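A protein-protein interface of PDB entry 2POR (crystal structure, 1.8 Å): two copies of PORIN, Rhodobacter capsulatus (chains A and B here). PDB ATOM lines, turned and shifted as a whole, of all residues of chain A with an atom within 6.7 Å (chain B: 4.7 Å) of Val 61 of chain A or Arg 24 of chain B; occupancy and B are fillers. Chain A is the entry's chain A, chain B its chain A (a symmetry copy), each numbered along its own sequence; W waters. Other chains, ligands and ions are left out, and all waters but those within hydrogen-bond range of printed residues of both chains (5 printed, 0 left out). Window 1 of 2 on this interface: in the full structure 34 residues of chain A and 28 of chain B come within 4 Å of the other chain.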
ATOM      1  N   GLY A  42       7.715 -15.090 -31.606  1.00  0.00           N
ATOM      2  CA  GLY A  42       6.357 -14.705 -31.321  1.00  0.00           C
ATOM      3  C   GLY A  42       5.533 -15.932 -30.906  1.00  0.00           C
ATOM      4  O   GLY A  42       6.085 -17.031 -30.827  1.00  0.00           O
ATOM      5  N   ALA A  43       4.263 -15.691 -30.656  1.00  0.00           N
ATOM      6  CA  ALA A  43       3.314 -16.728 -30.282  1.00  0.00           C
ATOM      7  C   ALA A  43       1.919 -16.171 -30.528  1.00  0.00           C
ATOM      8  O   ALA A  43       1.710 -14.946 -30.500  1.00  0.00           O
ATOM      9  CB  ALA A  43       3.489 -17.067 -28.804  1.00  0.00           C
ATOM     10  N   SER A  44       0.902 -16.967 -30.868  1.00  0.00           N
ATOM     11  CA  SER A  44      -0.452 -16.459 -30.898  1.00  0.00           C
ATOM     12  C   SER A  44      -1.432 -17.608 -30.615  1.00  0.00           C
ATOM     13  O   SER A  44      -1.085 -18.770 -30.858  1.00  0.00           O
ATOM     14  CB  SER A  44      -0.796 -15.862 -32.256  1.00  0.00           C
ATOM     15  OG  SER A  44      -0.538 -16.739 -33.311  1.00  0.00           O
ATOM     16  N   GLY A  52      -5.878 -24.980 -24.205  1.00  0.00           N
ATOM     17  CA  GLY A  52      -5.075 -25.764 -25.110  1.00  0.00           C
ATOM     18  C   GLY A  52      -3.747 -25.112 -25.409  1.00  0.00           C
ATOM     19  O   GLY A  52      -2.740 -25.797 -25.528  1.00  0.00           O
ATOM     20  N   ALA A  53      -3.695 -23.772 -25.508  1.00  0.00           N
ATOM     21  CA  ALA A  53      -2.432 -23.095 -25.811  1.00  0.00           C
ATOM     22  C   ALA A  53      -1.445 -23.303 -24.698  1.00  0.00           C
ATOM     23  O   ALA A  53      -0.241 -23.378 -24.943  1.00  0.00           O
ATOM     24  CB  ALA A  53      -2.705 -21.623 -25.994  1.00  0.00           C
ATOM     25  N   GLU A  54      -1.885 -23.455 -23.434  1.00  0.00           N
ATOM     26  CA  GLU A  54      -0.998 -23.736 -22.342  1.00  0.00           C
ATOM     27  C   GLU A  54      -0.386 -25.152 -22.371  1.00  0.00           C
ATOM     28  O   GLU A  54       0.555 -25.382 -21.614  1.00  0.00           O
ATOM     29  CB  GLU A  54      -1.796 -23.454 -21.084  1.00  0.00           C
ATOM     30  CG  GLU A  54      -0.945 -23.312 -19.798  1.00  0.00           C
ATOM     31  CD  GLU A  54      -0.811 -24.559 -18.898  1.00  0.00           C
ATOM     32  OE1 GLU A  54      -1.662 -25.441 -18.987  1.00  0.00           O
ATOM     33  OE2 GLU A  54       0.130 -24.660 -18.108  1.00  0.00           O
ATOM     34  N   THR A  55      -0.781 -26.148 -23.195  1.00  0.00           N
ATOM     35  CA  THR A  55      -0.117 -27.455 -23.238  1.00  0.00           C
ATOM     36  C   THR A  55       0.510 -27.702 -24.607  1.00  0.00           C
ATOM     37  O   THR A  55       1.140 -28.729 -24.814  1.00  0.00           O
ATOM     38  CB  THR A  55      -1.159 -28.593 -22.931  1.00  0.00           C
ATOM     39  OG1 THR A  55      -1.896 -28.785 -24.134  1.00  0.00           O
ATOM     40  CG2 THR A  55      -2.129 -28.253 -21.815  1.00  0.00           C
ATOM     41  N   GLY A  56       0.347 -26.841 -25.628  1.00  0.00           N
ATOM     42  CA  GLY A  56       0.933 -27.057 -26.953  1.00  0.00           C
ATOM     43  C   GLY A  56      -0.072 -27.548 -27.957  1.00  0.00           C
ATOM     44  O   GLY A  56       0.184 -27.710 -29.149  1.00  0.00           O
ATOM     45  N   ASP A  58      -3.008 -26.076 -28.850  1.00  0.00           N
ATOM     46  CA  ASP A  58      -3.588 -25.021 -29.669  1.00  0.00           C
ATOM     47  C   ASP A  58      -2.594 -23.842 -29.703  1.00  0.00           C
ATOM     48  O   ASP A  58      -1.750 -23.741 -28.817  1.00  0.00           O
ATOM     49  CB  ASP A  58      -4.864 -24.511 -29.076  1.00  0.00           C
ATOM     50  CG  ASP A  58      -6.030 -25.496 -29.201  1.00  0.00           C
ATOM     51  OD1 ASP A  58      -6.182 -26.132 -30.242  1.00  0.00           O
ATOM     52  OD2 ASP A  58      -6.782 -25.584 -28.242  1.00  0.00           O
ATOM     53  N   GLY A  59      -2.729 -22.983 -30.698  1.00  0.00           N
ATOM     54  CA  GLY A  59      -1.849 -21.822 -30.850  1.00  0.00           C
ATOM     55  C   GLY A  59      -0.494 -22.245 -31.346  1.00  0.00           C
ATOM     56  O   GLY A  59      -0.195 -23.443 -31.455  1.00  0.00           O
ATOM     57  N   THR A  60       0.382 -21.313 -31.733  1.00  0.00           N
ATOM     58  CA  THR A  60       1.750 -21.657 -32.152  1.00  0.00           C
ATOM     59  C   THR A  60       2.793 -20.716 -31.528  1.00  0.00           C
ATOM     60  O   THR A  60       2.396 -19.629 -31.087  1.00  0.00           O
ATOM     61  CB  THR A  60       1.948 -21.587 -33.677  1.00  0.00           C
ATOM     62  OG1 THR A  60       1.419 -20.357 -34.143  1.00  0.00           O
ATOM     63  CG2 THR A  60       1.271 -22.749 -34.393  1.00  0.00           C
ATOM     64  N   VAL A  61       4.046 -21.161 -31.410  1.00  0.00           N
ATOM     65  CA  VAL A  61       5.182 -20.392 -30.914  1.00  0.00           C
ATOM     66  C   VAL A  61       6.195 -20.440 -32.077  1.00  0.00           C
ATOM     67  O   VAL A  61       6.300 -21.476 -32.766  1.00  0.00           O
ATOM     68  CB  VAL A  61       5.769 -21.042 -29.639  1.00  0.00           C
ATOM     69  CG1 VAL A  61       6.980 -20.260 -29.135  1.00  0.00           C
ATOM     70  CG2 VAL A  61       4.729 -21.033 -28.558  1.00  0.00           C
ATOM     71  N   PHE A  62       6.929 -19.358 -32.408  1.00  0.00           N
ATOM     72  CA  PHE A  62       7.906 -19.428 -33.493  1.00  0.00           C
ATOM     73  C   PHE A  62       9.175 -18.623 -33.189  1.00  0.00           C
ATOM     74  O   PHE A  62       9.190 -17.742 -32.310  1.00  0.00           O
ATOM     75  CB  PHE A  62       7.300 -18.926 -34.795  1.00  0.00           C
ATOM     76  CG  PHE A  62       7.110 -17.409 -34.897  1.00  0.00           C
ATOM     77  CD1 PHE A  62       8.148 -16.599 -35.369  1.00  0.00           C
ATOM     78  CD2 PHE A  62       5.893 -16.856 -34.544  1.00  0.00           C
ATOM     79  CE1 PHE A  62       7.953 -15.235 -35.490  1.00  0.00           C
ATOM     80  CE2 PHE A  62       5.715 -15.484 -34.672  1.00  0.00           C
ATOM     81  CZ  PHE A  62       6.736 -14.673 -35.143  1.00  0.00           C
ATOM     82  N   LEU A  63      10.209 -18.982 -33.943  1.00  0.00           N
ATOM     83  CA  LEU A  63      11.518 -18.317 -33.935  1.00  0.00           C
ATOM     84  C   LEU A  63      11.922 -18.228 -35.382  1.00  0.00           C
ATOM     85  O   LEU A  63      11.824 -19.259 -36.053  1.00  0.00           O
ATOM     86  CB  LEU A  63      12.619 -19.116 -33.235  1.00  0.00           C
ATOM     87  CG  LEU A  63      14.013 -18.471 -33.169  1.00  0.00           C
ATOM     88  CD1 LEU A  63      13.990 -17.226 -32.291  1.00  0.00           C
ATOM     89  CD2 LEU A  63      14.966 -19.438 -32.532  1.00  0.00           C
ATOM     90  N   LYS A  69      11.986 -20.211 -40.635  1.00  0.00           N
ATOM     91  CA  LYS A  69      11.142 -20.032 -39.463  1.00  0.00           C
ATOM     92  C   LYS A  69      10.807 -21.417 -38.892  1.00  0.00           C
ATOM     93  O   LYS A  69      10.463 -22.312 -39.663  1.00  0.00           O
ATOM     94  CB  LYS A  69       9.878 -19.326 -39.904  1.00  0.00           C
ATOM     95  CG  LYS A  69       8.883 -19.045 -38.778  1.00  0.00           C
ATOM     96  CD  LYS A  69       7.665 -18.466 -39.468  1.00  0.00           C
ATOM     97  CE  LYS A  69       6.582 -18.214 -38.469  1.00  0.00           C
ATOM     98  NZ  LYS A  69       5.458 -17.540 -39.101  1.00  0.00           N
ATOM     99  N   ILE A  70      10.886 -21.582 -37.601  1.00  0.00           N
ATOM    100  CA  ILE A  70      10.549 -22.825 -36.912  1.00  0.00           C
ATOM    101  C   ILE A  70       9.321 -22.505 -36.074  1.00  0.00           C
ATOM    102  O   ILE A  70       9.376 -21.604 -35.230  1.00  0.00           O
ATOM    103  CB  ILE A  70      11.702 -23.236 -35.998  1.00  0.00           C
ATOM    104  CG1 ILE A  70      12.937 -23.537 -36.835  1.00  0.00           C
ATOM    105  CG2 ILE A  70      11.296 -24.470 -35.196  1.00  0.00           C
ATOM    106  CD1 ILE A  70      14.206 -23.572 -35.964  1.00  0.00           C
ATOM    107  N   GLU A  71       8.216 -23.226 -36.219  1.00  0.00           N
ATOM    108  CA  GLU A  71       6.981 -22.971 -35.497  1.00  0.00           C
ATOM    109  C   GLU A  71       6.564 -24.273 -34.767  1.00  0.00           C
ATOM    110  O   GLU A  71       6.662 -25.340 -35.403  1.00  0.00           O
ATOM    111  CB  GLU A  71       6.003 -22.566 -36.536  1.00  0.00           C
ATOM    112  CG  GLU A  71       4.702 -22.036 -36.004  1.00  0.00           C
ATOM    113  CD  GLU A  71       3.759 -21.550 -37.102  1.00  0.00           C
ATOM    114  OE1 GLU A  71       3.857 -22.064 -38.202  1.00  0.00           O
ATOM    115  OE2 GLU A  71       2.946 -20.649 -36.852  1.00  0.00           O
ATOM    116  N   MET A  72       6.098 -24.252 -33.511  1.00  0.00           N
ATOM    117  CA  MET A  72       5.722 -25.475 -32.807  1.00  0.00           C
ATOM    118  C   MET A  72       4.386 -25.208 -32.170  1.00  0.00           C
ATOM    119  O   MET A  72       4.171 -24.095 -31.657  1.00  0.00           O
ATOM    120  CB  MET A  72       6.753 -25.773 -31.767  1.00  0.00           C
ATOM    121  CG  MET A  72       6.547 -27.151 -31.102  1.00  0.00           C
ATOM    122  SD  MET A  72       7.867 -27.598 -29.969  1.00  0.00           S
ATOM    123  CE  MET A  72       9.138 -27.917 -31.135  1.00  0.00           C
ATOM    124  N   GLY A  73       3.454 -26.177 -32.245  1.00  0.00           N
ATOM    125  CA  GLY A  73       2.157 -26.092 -31.575  1.00  0.00           C
ATOM    126  C   GLY A  73       1.137 -26.680 -32.516  1.00  0.00           C
ATOM    127  O   GLY A  73       1.412 -27.671 -33.194  1.00  0.00           O
ATOM    128  N   ASP A  74       0.013 -26.011 -32.681  1.00  0.00           N
ATOM    129  CA  ASP A  74      -1.005 -26.445 -33.581  1.00  0.00           C
ATOM    130  C   ASP A  74      -0.686 -25.838 -34.949  1.00  0.00           C
ATOM    131  O   ASP A  74      -1.321 -24.892 -35.400  1.00  0.00           O
ATOM    132  CB  ASP A  74      -2.367 -26.002 -33.001  1.00  0.00           C
ATOM    133  CG  ASP A  74      -3.610 -26.461 -33.769  1.00  0.00           C
ATOM    134  OD1 ASP A  74      -3.493 -27.089 -34.840  1.00  0.00           O
ATOM    135  OD2 ASP A  74      -4.719 -26.173 -33.296  1.00  0.00           O
ATOM    136  N   PRO A 117       2.457 -30.927 -29.267  1.00  0.00           N
ATOM    137  CA  PRO A 117       2.564 -30.009 -30.389  1.00  0.00           C
ATOM    138  C   PRO A 117       3.202 -30.671 -31.610  1.00  0.00           C
ATOM    139  O   PRO A 117       3.935 -31.661 -31.462  1.00  0.00           O
ATOM    140  CB  PRO A 117       3.373 -28.862 -29.793  1.00  0.00           C
ATOM    141  CG  PRO A 117       4.331 -29.559 -28.850  1.00  0.00           C
ATOM    142  CD  PRO A 117       3.424 -30.611 -28.219  1.00  0.00           C
ATOM    143  N   ASP B   7       4.084 -15.016 -22.184  1.00  0.00           N
ATOM    144  CA  ASP B   7       5.305 -15.784 -22.327  1.00  0.00           C
ATOM    145  C   ASP B   7       5.002 -16.997 -23.203  1.00  0.00           C
ATOM    146  O   ASP B   7       3.839 -17.268 -23.526  1.00  0.00           O
ATOM    147  CB  ASP B   7       5.872 -16.228 -20.956  1.00  0.00           C
ATOM    148  CG  ASP B   7       4.897 -16.952 -20.034  1.00  0.00           C
ATOM    149  OD1 ASP B   7       4.337 -17.964 -20.423  1.00  0.00           O
ATOM    150  OD2 ASP B   7       4.663 -16.476 -18.946  1.00  0.00           O
ATOM    151  N   ALA B   8       6.052 -17.658 -23.663  1.00  0.00           N
ATOM    152  CA  ALA B   8       5.952 -18.830 -24.538  1.00  0.00           C
ATOM    153  C   ALA B   8       7.273 -19.574 -24.455  1.00  0.00           C
ATOM    154  O   ALA B   8       8.261 -19.051 -23.898  1.00  0.00           O
ATOM    155  CB  ALA B   8       5.689 -18.452 -26.000  1.00  0.00           C
ATOM    156  N   ARG B   9       7.304 -20.858 -24.842  1.00  0.00           N
ATOM    157  CA  ARG B   9       8.524 -21.643 -24.814  1.00  0.00           C
ATOM    158  C   ARG B   9       8.376 -22.759 -25.817  1.00  0.00           C
ATOM    159  O   ARG B   9       7.240 -23.100 -26.198  1.00  0.00           O
ATOM    160  CB  ARG B   9       8.771 -22.187 -23.404  1.00  0.00           C
ATOM    161  CG  ARG B   9       7.814 -23.289 -22.995  1.00  0.00           C
ATOM    162  CD  ARG B   9       7.924 -23.470 -21.521  1.00  0.00           C
ATOM    163  NE  ARG B   9       7.140 -24.642 -21.164  1.00  0.00           N
ATOM    164  CZ  ARG B   9       6.828 -24.969 -19.899  1.00  0.00           C
ATOM    165  NH1 ARG B   9       7.184 -24.226 -18.840  1.00  0.00           N
ATOM    166  NH2 ARG B   9       6.094 -26.083 -19.717  1.00  0.00           N
ATOM    167  N   MET B  10       9.455 -23.276 -26.368  1.00  0.00           N
ATOM    168  CA  MET B  10       9.387 -24.386 -27.317  1.00  0.00           C
ATOM    169  C   MET B  10      10.734 -25.074 -27.337  1.00  0.00           C
ATOM    170  O   MET B  10      11.754 -24.445 -27.043  1.00  0.00           O
ATOM    171  CB  MET B  10       9.003 -23.947 -28.730  1.00  0.00           C
ATOM    172  CG  MET B  10      10.005 -23.123 -29.482  1.00  0.00           C
ATOM    173  SD  MET B  10       9.428 -22.896 -31.161  1.00  0.00           S
ATOM    174  CE  MET B  10      10.564 -21.592 -31.423  1.00  0.00           C
ATOM    175  N   SER B  23       5.872 -27.382 -25.912  1.00  0.00           N
ATOM    176  CA  SER B  23       5.743 -25.951 -26.146  1.00  0.00           C
ATOM    177  C   SER B  23       4.494 -25.407 -25.475  1.00  0.00           C
ATOM    178  O   SER B  23       3.635 -26.194 -25.057  1.00  0.00           O
ATOM    179  CB  SER B  23       5.718 -25.738 -27.648  1.00  0.00           C
ATOM    180  OG  SER B  23       4.592 -26.259 -28.322  1.00  0.00           O
ATOM    181  N   ARG B  24       4.343 -24.108 -25.241  1.00  0.00           N
ATOM    182  CA  ARG B  24       3.131 -23.521 -24.698  1.00  0.00           C
ATOM    183  C   ARG B  24       3.204 -22.009 -24.914  1.00  0.00           C
ATOM    184  O   ARG B  24       4.291 -21.499 -25.181  1.00  0.00           O
ATOM    185  CB  ARG B  24       2.978 -23.714 -23.201  1.00  0.00           C
ATOM    186  CG  ARG B  24       3.892 -23.038 -22.260  1.00  0.00           C
ATOM    187  CD  ARG B  24       3.362 -23.170 -20.890  1.00  0.00           C
ATOM    188  NE  ARG B  24       4.270 -22.408 -20.038  1.00  0.00           N
ATOM    189  CZ  ARG B  24       4.377 -22.485 -18.718  1.00  0.00           C
ATOM    190  NH1 ARG B  24       3.662 -23.323 -17.975  1.00  0.00           N
ATOM    191  NH2 ARG B  24       5.176 -21.615 -18.107  1.00  0.00           N
ATOM    192  N   SER B  25       2.109 -21.296 -24.789  1.00  0.00           N
ATOM    193  CA  SER B  25       2.122 -19.846 -24.744  1.00  0.00           C
ATOM    194  C   SER B  25       1.040 -19.476 -23.758  1.00  0.00           C
ATOM    195  O   SER B  25       0.039 -20.199 -23.577  1.00  0.00           O
ATOM    196  CB  SER B  25       1.866 -19.234 -26.142  1.00  0.00           C
ATOM    197  OG  SER B  25       0.779 -19.720 -26.874  1.00  0.00           O
ATOM    198  N   ARG B  26       1.211 -18.358 -23.039  1.00  0.00           N
ATOM    199  CA  ARG B  26       0.286 -17.879 -22.010  1.00  0.00           C
ATOM    200  C   ARG B  26       0.168 -16.343 -22.124  1.00  0.00           C
ATOM    201  O   ARG B  26       1.094 -15.706 -22.652  1.00  0.00           O
ATOM    202  CB  ARG B  26       0.809 -18.210 -20.610  1.00  0.00           C
ATOM    203  CG  ARG B  26       1.125 -19.702 -20.491  1.00  0.00           C
ATOM    204  CD  ARG B  26       1.376 -20.081 -19.066  1.00  0.00           C
ATOM    205  NE  ARG B  26       2.480 -19.324 -18.565  1.00  0.00           N
ATOM    206  CZ  ARG B  26       2.855 -19.332 -17.298  1.00  0.00           C
ATOM    207  NH1 ARG B  26       2.251 -20.048 -16.370  1.00  0.00           N
ATOM    208  NH2 ARG B  26       3.855 -18.542 -16.914  1.00  0.00           N
ATOM    209  N   PHE B 299      10.452 -17.253 -24.037  1.00  0.00           N
ATOM    210  CA  PHE B 299      10.189 -15.919 -24.562  1.00  0.00           C
ATOM    211  C   PHE B 299       9.333 -15.169 -23.578  1.00  0.00           C
ATOM    212  O   PHE B 299       8.463 -15.760 -22.918  1.00  0.00           O
ATOM    213  CB  PHE B 299       9.435 -16.023 -25.860  1.00  0.00           C
ATOM    214  CG  PHE B 299      10.109 -16.783 -26.982  1.00  0.00           C
ATOM    215  CD1 PHE B 299      11.442 -16.578 -27.297  1.00  0.00           C
ATOM    216  CD2 PHE B 299       9.374 -17.673 -27.729  1.00  0.00           C
ATOM    217  CE1 PHE B 299      12.031 -17.252 -28.347  1.00  0.00           C
ATOM    218  CE2 PHE B 299       9.979 -18.336 -28.780  1.00  0.00           C
ATOM    219  CZ  PHE B 299      11.302 -18.133 -29.096  1.00  0.00           C
HETATM  220  O   HOH W   1       2.828 -24.214 -28.743  1.00  0.00           O
HETATM  221  O   HOH W   2       3.797 -29.462 -25.152  1.00  0.00           O
HETATM  222  O   HOH W   3       3.420 -27.243 -22.358  1.00  0.00           O
HETATM  223  O   HOH W   4       0.891 -22.566 -16.500  1.00  0.00           O
HETATM  224  O   HOH W   5       0.687 -22.959 -27.726  1.00  0.00           O
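No position is printed for both chains.
Of the 19 pairs that touch across the chains among the printed residues, none has its exchanged pair printed and touching as well.
N of Ile 70 of chain A sits at hydrogen-bond distance from O of Leu 63 of chain A (2.9 Å).
OG1 of Thr 55 of chain A lies within hydrogen-bond range of O of Gly 52 of chain A, 3.4 Å away.
The backbone NH of Arg 9 of chain B is in hydrogen-bond range of the backbone carbonyl oxygen of Arg 24 of chain B (3.1 Å).
N of Met 72 of chain A sits at hydrogen-bond distance from O of Val 61 of chain A, at 2.9 Å.
The backbone carbonyl oxygen of Gly 42 of chain A lies within hydrogen-bond range of the backbone NH of Phe 62 of chain A, 2.9 Å away.
The backbone NH (N) of Phe 299 of chain B lies within hydrogen-bond range of the backbone carbonyl oxygen (O) of Ala 8 of chain B (2.8 Å).
Of the 21 printed residues of chain A, 11 touch a printed residue of chain B.
Among the printed residues, Asp or Glu carboxylates within 4 Å of a Lys or Arg side-chain nitrogen of the other chain: Glu 54 of chain A with Arg 24 of chain B.
Ala 8 of chain B touches Ala 43 of chain A.
Arg 24 of chain B touches Ala 53 of chain A.
Glu 54 of chain A touches Ser 25 of chain B (N to O, 3.8 Å).
Thr 55 of chain A touches Ser 23 of chain B.
Val 61 of chain A touches Arg 24 of chain B.
CG1 of Val 61 of chain A touches CE2 of Phe 299 of chain B, 3.6 Å away.
Phe 299 of chain B touches Phe 62 of chain A (CE2 to O, 3.7 Å).
Met 10 of chain B touches Ile 70 of chain A (CE to O, 3.99 Å).
CG of Met 72 of chain A touches OG of Ser 23 of chain B (3.5 Å).
Ser 23 of chain B touches Pro 117 of chain A (OG to CB, 3.2 Å).
Water W1 bridges the side-chain hydroxyl (OG) of Ser 23 of chain B (2.7 Å) and the backbone carbonyl oxygen (O) of Met 72 of chain A (3.2 Å).
Water W4 lies within hydrogen-bond range of OE2 of Glu 54 of chain A (2.7 Å), NH1 of Arg 26 of chain B (2.9 Å) and NH1 of Arg 24 of chain B (3.2 Å).
Water W2 bridges O of Thr 55 of chain A (2.8 Å) and N of Ser 23 of chain B (3.0 Å).
Water W5 lies within hydrogen-bond range of O of Asp 58 of chain A, O of Ala 53 of chain A and OG of Ser 25 of chain B.
Water W3 bridges the backbone carbonyl oxygen (O) of Ser 23 of chain B (2.9 Å) and the backbone carbonyl oxygen (O) of Glu 54 of chain A (3.5 Å).
The side-chain sulfur (SD) of Met 10 of chain B sits close to the backbone carbonyl oxygen (O) of Val 61 of chain A, 3.8 Å away.
The backbone NH (N) of Ser 25 of chain B is in hydrogen-bond range of the backbone carbonyl oxygen (O) of Ala 53 of chain A (3.1 Å).
The guanidinium group (NH1) of Arg 24 of chain B lies within salt-bridge range of the side-chain carboxylate (OE2) of Glu 54 of chain A.
N of Gly 56 of chain A lies within hydrogen-bond range of O of Ser 23 of chain B, 3.4 Å away.
Printed residues of chain B within 4 Å of Ala 43 of chain A: Ala 8 and Ser 25.
Printed residues of chain B within 4 Å of Leu 63 of chain A: Met 10.
Asp 74 of chain A touches none of the printed residues of chain B.
Arg 9 of chain B touches none of the printed residues of chain A.
Printed residues of chain A within 4 Å of Met 10 of chain B: Val 61 (3.8 Å), Phe 62 (3.7 Å), Leu 63 (3.6 Å), Ile 70 (3.99 Å) and Met 72 (3.97 Å).
Arg 24 of chain B touches three residues of chain A.
The nearest printed residue of chain B that does not touch Val 61 of chain A is Arg 9 of chain B (4.02 Å).
The nearest residue of chain A that does not touch Arg 24 of chain B is Gly 56 of chain A (4.4 Å).
The nearest printed residue of chain A that does not touch Ser 25 of chain B is Val 61 of chain A (4.2 Å).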
